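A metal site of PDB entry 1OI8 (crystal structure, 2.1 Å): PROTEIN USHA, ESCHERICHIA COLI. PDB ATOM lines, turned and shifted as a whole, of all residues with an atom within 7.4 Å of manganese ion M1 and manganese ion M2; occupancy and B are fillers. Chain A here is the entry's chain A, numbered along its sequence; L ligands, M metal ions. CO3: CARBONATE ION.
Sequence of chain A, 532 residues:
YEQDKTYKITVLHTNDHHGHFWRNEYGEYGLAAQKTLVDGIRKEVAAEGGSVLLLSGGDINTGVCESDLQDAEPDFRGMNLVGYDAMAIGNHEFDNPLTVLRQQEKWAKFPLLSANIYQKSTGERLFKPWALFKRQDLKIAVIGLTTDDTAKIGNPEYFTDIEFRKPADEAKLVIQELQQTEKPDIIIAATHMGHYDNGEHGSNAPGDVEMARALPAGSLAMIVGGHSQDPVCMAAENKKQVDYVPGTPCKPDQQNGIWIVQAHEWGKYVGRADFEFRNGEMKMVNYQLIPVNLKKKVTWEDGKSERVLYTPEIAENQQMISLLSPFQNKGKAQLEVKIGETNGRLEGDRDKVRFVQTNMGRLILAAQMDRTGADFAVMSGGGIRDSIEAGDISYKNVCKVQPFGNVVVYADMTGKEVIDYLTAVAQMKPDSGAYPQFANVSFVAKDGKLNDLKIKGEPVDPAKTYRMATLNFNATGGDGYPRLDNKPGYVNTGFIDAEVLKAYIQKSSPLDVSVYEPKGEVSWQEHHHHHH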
ATOM      1  N   ASN A  15       0.505  10.347 -28.143  1.00  0.00           N
ATOM      2  CA  ASN A  15      -0.909  10.676 -28.157  1.00  0.00           C
ATOM      3  C   ASN A  15      -1.117  12.169 -28.352  1.00  0.00           C
ATOM      4  O   ASN A  15      -0.214  12.964 -28.117  1.00  0.00           O
ATOM      5  CB  ASN A  15      -1.557  10.253 -26.859  1.00  0.00           C
ATOM      6  CG  ASN A  15      -0.883  10.883 -25.648  1.00  0.00           C
ATOM      7  OD1 ASN A  15       0.141  10.391 -25.160  1.00  0.00           O
ATOM      8  ND2 ASN A  15      -1.457  11.991 -25.160  1.00  0.00           N
ATOM      9  N   ASP A  16      -2.339  12.521 -28.751  1.00  0.00           N
ATOM     10  CA  ASP A  16      -2.736  13.923 -28.872  1.00  0.00           C
ATOM     11  C   ASP A  16      -1.761  14.739 -29.690  1.00  0.00           C
ATOM     12  O   ASP A  16      -1.338  15.831 -29.320  1.00  0.00           O
ATOM     13  CB  ASP A  16      -2.933  14.471 -27.475  1.00  0.00           C
ATOM     14  CG  ASP A  16      -4.097  13.859 -26.824  1.00  0.00           C
ATOM     15  OD1 ASP A  16      -5.215  14.340 -27.092  1.00  0.00           O
ATOM     16  OD2 ASP A  16      -3.981  12.827 -26.137  1.00  0.00           O
ATOM     17  N   HIS A  17      -1.406  14.157 -30.822  1.00  0.00           N
ATOM     18  CA  HIS A  17      -0.491  14.729 -31.815  1.00  0.00           C
ATOM     19  C   HIS A  17      -0.991  16.104 -32.306  1.00  0.00           C
ATOM     20  O   HIS A  17      -0.231  17.058 -32.414  1.00  0.00           O
ATOM     21  CB  HIS A  17      -0.338  13.719 -32.948  1.00  0.00           C
ATOM     22  CG  HIS A  17       0.436  14.221 -34.113  1.00  0.00           C
ATOM     23  ND1 HIS A  17       1.783  14.462 -34.047  1.00  0.00           N
ATOM     24  CD2 HIS A  17       0.039  14.526 -35.377  1.00  0.00           C
ATOM     25  CE1 HIS A  17       2.186  14.914 -35.230  1.00  0.00           C
ATOM     26  NE2 HIS A  17       1.149  14.941 -36.055  1.00  0.00           N
ATOM     27  N   HIS A  18      -2.267  16.189 -32.624  1.00  0.00           N
ATOM     28  CA  HIS A  18      -2.943  17.462 -32.864  1.00  0.00           C
ATOM     29  C   HIS A  18      -2.268  18.327 -33.898  1.00  0.00           C
ATOM     30  O   HIS A  18      -1.965  19.484 -33.653  1.00  0.00           O
ATOM     31  CB  HIS A  18      -3.065  18.218 -31.578  1.00  0.00           C
ATOM     32  CG  HIS A  18      -4.192  17.763 -30.718  1.00  0.00           C
ATOM     33  ND1 HIS A  18      -5.501  17.703 -31.158  1.00  0.00           N
ATOM     34  CD2 HIS A  18      -4.211  17.362 -29.419  1.00  0.00           C
ATOM     35  CE1 HIS A  18      -6.279  17.301 -30.146  1.00  0.00           C
ATOM     36  NE2 HIS A  18      -5.516  17.074 -29.103  1.00  0.00           N
ATOM     37  N   GLY A  57      -2.490   7.169 -28.855  1.00  0.00           N
ATOM     38  CA  GLY A  57      -3.751   7.348 -28.173  1.00  0.00           C
ATOM     39  C   GLY A  57      -4.694   8.317 -28.834  1.00  0.00           C
ATOM     40  O   GLY A  57      -5.633   8.753 -28.197  1.00  0.00           O
ATOM     41  N   GLY A  58      -4.430   8.698 -30.075  1.00  0.00           N
ATOM     42  CA  GLY A  58      -5.406   9.415 -30.890  1.00  0.00           C
ATOM     43  C   GLY A  58      -5.327  10.936 -30.722  1.00  0.00           C
ATOM     44  O   GLY A  58      -4.382  11.486 -30.121  1.00  0.00           O
ATOM     45  N   ASP A  59      -6.330  11.614 -31.282  1.00  0.00           N
ATOM     46  CA  ASP A  59      -6.388  13.081 -31.376  1.00  0.00           C
ATOM     47  C   ASP A  59      -5.202  13.532 -32.214  1.00  0.00           C
ATOM     48  O   ASP A  59      -4.313  14.298 -31.788  1.00  0.00           O
ATOM     49  CB  ASP A  59      -6.400  13.754 -30.020  1.00  0.00           C
ATOM     50  CG  ASP A  59      -7.785  14.046 -29.497  1.00  0.00           C
ATOM     51  OD1 ASP A  59      -8.847  13.603 -30.067  1.00  0.00           O
ATOM     52  OD2 ASP A  59      -7.901  14.789 -28.510  1.00  0.00           O
ATOM     53  N   ILE A  60      -5.219  13.027 -33.434  1.00  0.00           N
ATOM     54  CA  ILE A  60      -4.276  13.434 -34.485  1.00  0.00           C
ATOM     55  C   ILE A  60      -4.758  14.776 -35.130  1.00  0.00           C
ATOM     56  O   ILE A  60      -3.979  15.670 -35.383  1.00  0.00           O
ATOM     57  CB  ILE A  60      -4.146  12.326 -35.501  1.00  0.00           C
ATOM     58  CG1 ILE A  60      -3.849  10.950 -34.832  1.00  0.00           C
ATOM     59  CG2 ILE A  60      -3.110  12.692 -36.627  1.00  0.00           C
ATOM     60  CD1 ILE A  60      -2.584  10.827 -34.047  1.00  0.00           C
ATOM     61  N   ASN A  61      -6.054  14.876 -35.422  1.00  0.00           N
ATOM     62  CA  ASN A  61      -6.667  16.082 -35.933  1.00  0.00           C
ATOM     63  C   ASN A  61      -6.686  17.247 -34.945  1.00  0.00           C
ATOM     64  O   ASN A  61      -6.919  17.051 -33.735  1.00  0.00           O
ATOM     65  CB  ASN A  61      -8.172  15.823 -36.285  1.00  0.00           C
ATOM     66  CG  ASN A  61      -8.362  14.930 -37.455  1.00  0.00           C
ATOM     67  OD1 ASN A  61      -8.451  15.399 -38.565  1.00  0.00           O
ATOM     68  ND2 ASN A  61      -8.396  13.616 -37.212  1.00  0.00           N
ATOM     69  N   THR A  62      -6.521  18.438 -35.531  1.00  0.00           N
ATOM     70  CA  THR A  62      -6.880  19.741 -34.986  1.00  0.00           C
ATOM     71  C   THR A  62      -5.757  20.304 -34.092  1.00  0.00           C
ATOM     72  O   THR A  62      -5.411  19.698 -33.112  1.00  0.00           O
ATOM     73  CB  THR A  62      -8.174  19.688 -34.253  1.00  0.00           C
ATOM     74  OG1 THR A  62      -9.192  19.195 -35.131  1.00  0.00           O
ATOM     75  CG2 THR A  62      -8.665  21.062 -33.835  1.00  0.00           C
ATOM     76  N   GLY A  90      -9.628   9.332 -31.335  1.00  0.00           N
ATOM     77  CA  GLY A  90      -9.912  10.357 -30.365  1.00  0.00           C
ATOM     78  C   GLY A  90     -11.177  11.157 -30.680  1.00  0.00           C
ATOM     79  O   GLY A  90     -11.790  11.023 -31.742  1.00  0.00           O
ATOM     80  N   ASN A  91     -11.535  12.034 -29.763  1.00  0.00           N
ATOM     81  CA  ASN A  91     -12.743  12.859 -29.986  1.00  0.00           C
ATOM     82  C   ASN A  91     -12.580  13.817 -31.121  1.00  0.00           C
ATOM     83  O   ASN A  91     -13.525  14.034 -31.882  1.00  0.00           O
ATOM     84  CB  ASN A  91     -13.187  13.585 -28.709  1.00  0.00           C
ATOM     85  CG  ASN A  91     -12.099  14.372 -28.067  1.00  0.00           C
ATOM     86  OD1 ASN A  91     -11.197  13.802 -27.544  1.00  0.00           O
ATOM     87  ND2 ASN A  91     -12.208  15.737 -28.097  1.00  0.00           N
ATOM     88  N   HIS A  92     -11.371  14.312 -31.307  1.00  0.00           N
ATOM     89  CA  HIS A  92     -11.105  15.217 -32.393  1.00  0.00           C
ATOM     90  C   HIS A  92     -11.054  14.590 -33.753  1.00  0.00           C
ATOM     91  O   HIS A  92     -11.046  15.319 -34.737  1.00  0.00           O
ATOM     92  CB  HIS A  92      -9.870  16.113 -32.136  1.00  0.00           C
ATOM     93  CG  HIS A  92     -10.093  17.150 -31.094  1.00  0.00           C
ATOM     94  ND1 HIS A  92     -10.478  18.439 -31.386  1.00  0.00           N
ATOM     95  CD2 HIS A  92     -10.025  17.083 -29.741  1.00  0.00           C
ATOM     96  CE1 HIS A  92     -10.601  19.134 -30.268  1.00  0.00           C
ATOM     97  NE2 HIS A  92     -10.339  18.335 -29.248  1.00  0.00           N
ATOM     98  N   THR A 147     -13.411   8.044 -25.447  1.00  0.00           N
ATOM     99  CA  THR A 147     -14.197   8.575 -24.373  1.00  0.00           C
ATOM    100  C   THR A 147     -15.626   8.818 -24.821  1.00  0.00           C
ATOM    101  O   THR A 147     -15.863   9.326 -25.919  1.00  0.00           O
ATOM    102  CB  THR A 147     -13.617   9.876 -23.797  1.00  0.00           C
ATOM    103  OG1 THR A 147     -14.521  10.423 -22.790  1.00  0.00           O
ATOM    104  CG2 THR A 147     -13.539  10.981 -24.873  1.00  0.00           C
ATOM    105  N   THR A 150     -17.072  12.366 -26.089  1.00  0.00           N
ATOM    106  CA  THR A 150     -17.100  12.794 -27.479  1.00  0.00           C
ATOM    107  C   THR A 150     -18.449  13.318 -27.897  1.00  0.00           C
ATOM    108  O   THR A 150     -18.536  14.347 -28.573  1.00  0.00           O
ATOM    109  CB  THR A 150     -16.699  11.664 -28.402  1.00  0.00           C
ATOM    110  OG1 THR A 150     -15.387  11.167 -28.032  1.00  0.00           O
ATOM    111  CG2 THR A 150     -16.541  12.204 -29.828  1.00  0.00           C
ATOM    112  N   ILE A 153     -19.111  16.726 -26.343  1.00  0.00           N
ATOM    113  CA  ILE A 153     -18.307  17.871 -26.702  1.00  0.00           C
ATOM    114  C   ILE A 153     -18.354  18.236 -28.192  1.00  0.00           C
ATOM    115  O   ILE A 153     -18.235  19.416 -28.499  1.00  0.00           O
ATOM    116  CB  ILE A 153     -16.816  17.846 -26.211  1.00  0.00           C
ATOM    117  CG1 ILE A 153     -15.913  17.189 -27.188  1.00  0.00           C
ATOM    118  CG2 ILE A 153     -16.569  17.188 -24.810  1.00  0.00           C
ATOM    119  CD1 ILE A 153     -14.628  17.849 -27.192  1.00  0.00           C
ATOM    120  N   HIS A 192      -8.436   6.713 -25.739  1.00  0.00           N
ATOM    121  CA  HIS A 192      -8.519   8.130 -25.635  1.00  0.00           C
ATOM    122  C   HIS A 192      -9.576   8.454 -24.601  1.00  0.00           C
ATOM    123  O   HIS A 192     -10.736   8.754 -24.943  1.00  0.00           O
ATOM    124  CB  HIS A 192      -8.894   8.705 -26.968  1.00  0.00           C
ATOM    125  CG  HIS A 192      -8.662  10.166 -27.065  1.00  0.00           C
ATOM    126  ND1 HIS A 192      -7.558  10.678 -27.694  1.00  0.00           N
ATOM    127  CD2 HIS A 192      -9.278  11.217 -26.467  1.00  0.00           C
ATOM    128  CE1 HIS A 192      -7.563  11.998 -27.580  1.00  0.00           C
ATOM    129  NE2 HIS A 192      -8.605  12.358 -26.861  1.00  0.00           N
ATOM    130  N   MET A 193      -9.158   8.338 -23.331  1.00  0.00           N
ATOM    131  CA  MET A 193     -10.085   8.425 -22.178  1.00  0.00           C
ATOM    132  C   MET A 193      -9.700   9.340 -21.022  1.00  0.00           C
ATOM    133  O   MET A 193     -10.589   9.826 -20.330  1.00  0.00           O
ATOM    134  CB  MET A 193     -10.357   7.024 -21.625  1.00  0.00           C
ATOM    135  CG  MET A 193     -11.223   6.194 -22.516  1.00  0.00           C
ATOM    136  SD  MET A 193     -11.091   4.397 -22.071  1.00  0.00           S
ATOM    137  CE  MET A 193     -11.598   4.424 -20.363  1.00  0.00           C
ATOM    138  N   GLY A 226      -4.452   8.793 -23.563  1.00  0.00           N
ATOM    139  CA  GLY A 226      -4.502  10.085 -24.190  1.00  0.00           C
ATOM    140  C   GLY A 226      -5.585  10.932 -23.563  1.00  0.00           C
ATOM    141  O   GLY A 226      -6.081  10.626 -22.465  1.00  0.00           O
ATOM    142  N   HIS A 227      -5.871  12.020 -24.250  1.00  0.00           N
ATOM    143  CA  HIS A 227      -7.048  12.902 -24.038  1.00  0.00           C
ATOM    144  C   HIS A 227      -6.851  13.878 -22.913  1.00  0.00           C
ATOM    145  O   HIS A 227      -7.017  15.055 -23.105  1.00  0.00           O
ATOM    146  CB  HIS A 227      -8.314  12.116 -23.776  1.00  0.00           C
ATOM    147  CG  HIS A 227      -9.558  12.957 -23.633  1.00  0.00           C
ATOM    148  ND1 HIS A 227     -10.151  13.623 -24.683  1.00  0.00           N
ATOM    149  CD2 HIS A 227     -10.318  13.224 -22.531  1.00  0.00           C
ATOM    150  CE1 HIS A 227     -11.236  14.263 -24.245  1.00  0.00           C
ATOM    151  NE2 HIS A 227     -11.379  13.994 -22.954  1.00  0.00           N
ATOM    152  N   SER A 228      -6.472  13.406 -21.728  1.00  0.00           N
ATOM    153  CA  SER A 228      -6.174  14.367 -20.645  1.00  0.00           C
ATOM    154  C   SER A 228      -4.939  15.217 -20.980  1.00  0.00           C
ATOM    155  O   SER A 228      -4.813  16.372 -20.522  1.00  0.00           O
ATOM    156  CB  SER A 228      -6.038  13.650 -19.294  1.00  0.00           C
ATOM    157  OG  SER A 228      -5.130  12.574 -19.320  1.00  0.00           O
ATOM    158  N   GLN A 229      -4.073  14.693 -21.834  1.00  0.00           N
ATOM    159  CA  GLN A 229      -2.845  15.370 -22.223  1.00  0.00           C
ATOM    160  C   GLN A 229      -1.930  15.601 -21.028  1.00  0.00           C
ATOM    161  O   GLN A 229      -1.615  16.709 -20.683  1.00  0.00           O
ATOM    162  CB  GLN A 229      -3.122  16.643 -23.079  1.00  0.00           C
ATOM    163  CG  GLN A 229      -3.808  16.304 -24.448  1.00  0.00           C
ATOM    164  CD  GLN A 229      -4.136  17.490 -25.383  1.00  0.00           C
ATOM    165  OE1 GLN A 229      -5.163  17.412 -26.004  1.00  0.00           O
ATOM    166  NE2 GLN A 229      -3.250  18.532 -25.518  1.00  0.00           N
ATOM    167  N   HIS A 264       1.911  12.912 -22.870  1.00  0.00           N
ATOM    168  CA  HIS A 264       1.585  14.359 -22.930  1.00  0.00           C
ATOM    169  C   HIS A 264       0.880  14.758 -24.219  1.00  0.00           C
ATOM    170  O   HIS A 264      -0.367  14.636 -24.302  1.00  0.00           O
ATOM    171  CB  HIS A 264       2.779  15.257 -22.588  1.00  0.00           C
ATOM    172  CG  HIS A 264       2.443  16.658 -22.160  1.00  0.00           C
ATOM    173  ND1 HIS A 264       3.417  17.607 -21.947  1.00  0.00           N
ATOM    174  CD2 HIS A 264       1.266  17.245 -21.823  1.00  0.00           C
ATOM    175  CE1 HIS A 264       2.852  18.741 -21.565  1.00  0.00           C
ATOM    176  NE2 HIS A 264       1.553  18.545 -21.453  1.00  0.00           N
ATOM    177  N   GLU A 265       1.607  15.240 -25.200  1.00  0.00           N
ATOM    178  CA  GLU A 265       0.955  15.787 -26.380  1.00  0.00           C
ATOM    179  C   GLU A 265       1.938  16.208 -27.442  1.00  0.00           C
ATOM    180  O   GLU A 265       3.119  16.486 -27.157  1.00  0.00           O
ATOM    181  CB  GLU A 265       0.099  17.025 -25.995  1.00  0.00           C
ATOM    182  CG  GLU A 265       0.961  18.208 -25.537  1.00  0.00           C
ATOM    183  CD  GLU A 265       0.234  19.339 -24.809  1.00  0.00           C
ATOM    184  OE1 GLU A 265      -0.946  19.234 -24.379  1.00  0.00           O
ATOM    185  OE2 GLU A 265       0.924  20.328 -24.580  1.00  0.00           O
ATOM    186  N   TRP A 266       1.404  16.326 -28.660  1.00  0.00           N
ATOM    187  CA  TRP A 266       2.031  17.052 -29.794  1.00  0.00           C
ATOM    188  C   TRP A 266       3.321  16.485 -30.323  1.00  0.00           C
ATOM    189  O   TRP A 266       4.146  17.185 -30.965  1.00  0.00           O
ATOM    190  CB  TRP A 266       2.272  18.505 -29.471  1.00  0.00           C
ATOM    191  CG  TRP A 266       1.135  19.349 -29.011  1.00  0.00           C
ATOM    192  CD1 TRP A 266      -0.176  19.027 -28.986  1.00  0.00           C
ATOM    193  CD2 TRP A 266       1.222  20.705 -28.591  1.00  0.00           C
ATOM    194  NE1 TRP A 266      -0.926  20.089 -28.544  1.00  0.00           N
ATOM    195  CE2 TRP A 266      -0.093  21.135 -28.278  1.00  0.00           C
ATOM    196  CE3 TRP A 266       2.273  21.592 -28.422  1.00  0.00           C
ATOM    197  CZ2 TRP A 266      -0.379  22.398 -27.777  1.00  0.00           C
ATOM    198  CZ3 TRP A 266       2.003  22.886 -27.920  1.00  0.00           C
ATOM    199  CH2 TRP A 266       0.694  23.268 -27.597  1.00  0.00           C
HETATM  200  C   CO3 L   1      -8.861  16.738 -26.159  1.00  0.00           C
HETATM  201  O1  CO3 L   1      -7.986  15.705 -25.736  1.00  0.00           O
HETATM  202  O2  CO3 L   1      -8.405  17.896 -26.599  1.00  0.00           O
HETATM  203  O3  CO3 L   1     -10.151  16.521 -26.350  1.00  0.00           O
HETATM  204 MN    MN M   1      -6.458  16.080 -27.302  1.00  0.00          MN
HETATM  205 MN    MN M   2      -9.309  14.343 -26.581  1.00  0.00          MN
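O1 of the ligand binds manganese ion M2.
Manganese ion M2 is bound by NE2 of His 192 (2.1 Å).
Manganese ion M2 is bound by the side-chain amide oxygen (OD1) of Asn 91 (2.2 Å).
A ring nitrogen (ND1) of His 227 is bound to manganese ion M2.
Manganese ion M2 is bound by O3 of the ligand (2.3 Å).
The side-chain carboxylate (OD2) of Asp 59 is bound to manganese ion M2, at 2.4 Å.
The backbone carbonyl oxygen (O) of His 192 is in hydrogen-bond range of the backbone NH (N) of Thr 147, at 2.8 Å.
OD2 of Asp 16 is in hydrogen-bond range of N of His 227 (2.8 Å).
The backbone NH of Asp 16 lies within hydrogen-bond range of the backbone carbonyl oxygen of Gly 58 (2.7 Å).
The side-chain amide nitrogen (ND2) of Asn 91 lies close to a ring nitrogen (NE2) of His 92 (3.4 Å).
A ring nitrogen (ND1) of His 18 sits at hydrogen-bond distance from the backbone carbonyl oxygen (O) of Asn 61, 3.0 Å away.
N of His 18 sits close to O of Ile 60, 3.3 Å away.
NE2 of Gln 229 lies within hydrogen-bond range of OE1 of Glu 265 (2.7 Å).
The side-chain carboxylate of Asp 59 is in hydrogen-bond range of the backbone NH of His 92, at 2.9 Å.
Four residues have an atom within 4 Å of manganese ion M2: Asp 59, Asn 91, His 192 and His 227.
Four residues have an atom within 4 Å of manganese ion M1: Asp 16, His 18, Asp 59 and Gln 229.
The nearest printed residue that does not touch manganese ion M1 is His 192 (4.2 Å).
Manganese ion M1 is bound by the side-chain carboxylate (OD1) of Asp 16 (2.1 Å), an oxygen (O1) of the ligand (2.2 Å), a ring nitrogen (NE2) of His 18 (2.3 Å), the side-chain amide oxygen (OE1) of Gln 229 (2.3 Å) and the side-chain carboxylate (OD2) of Asp 59 (2.3 Å).
Slightly farther from manganese ion M1 lies an oxygen (O2) of the ligand (2.8 Å).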
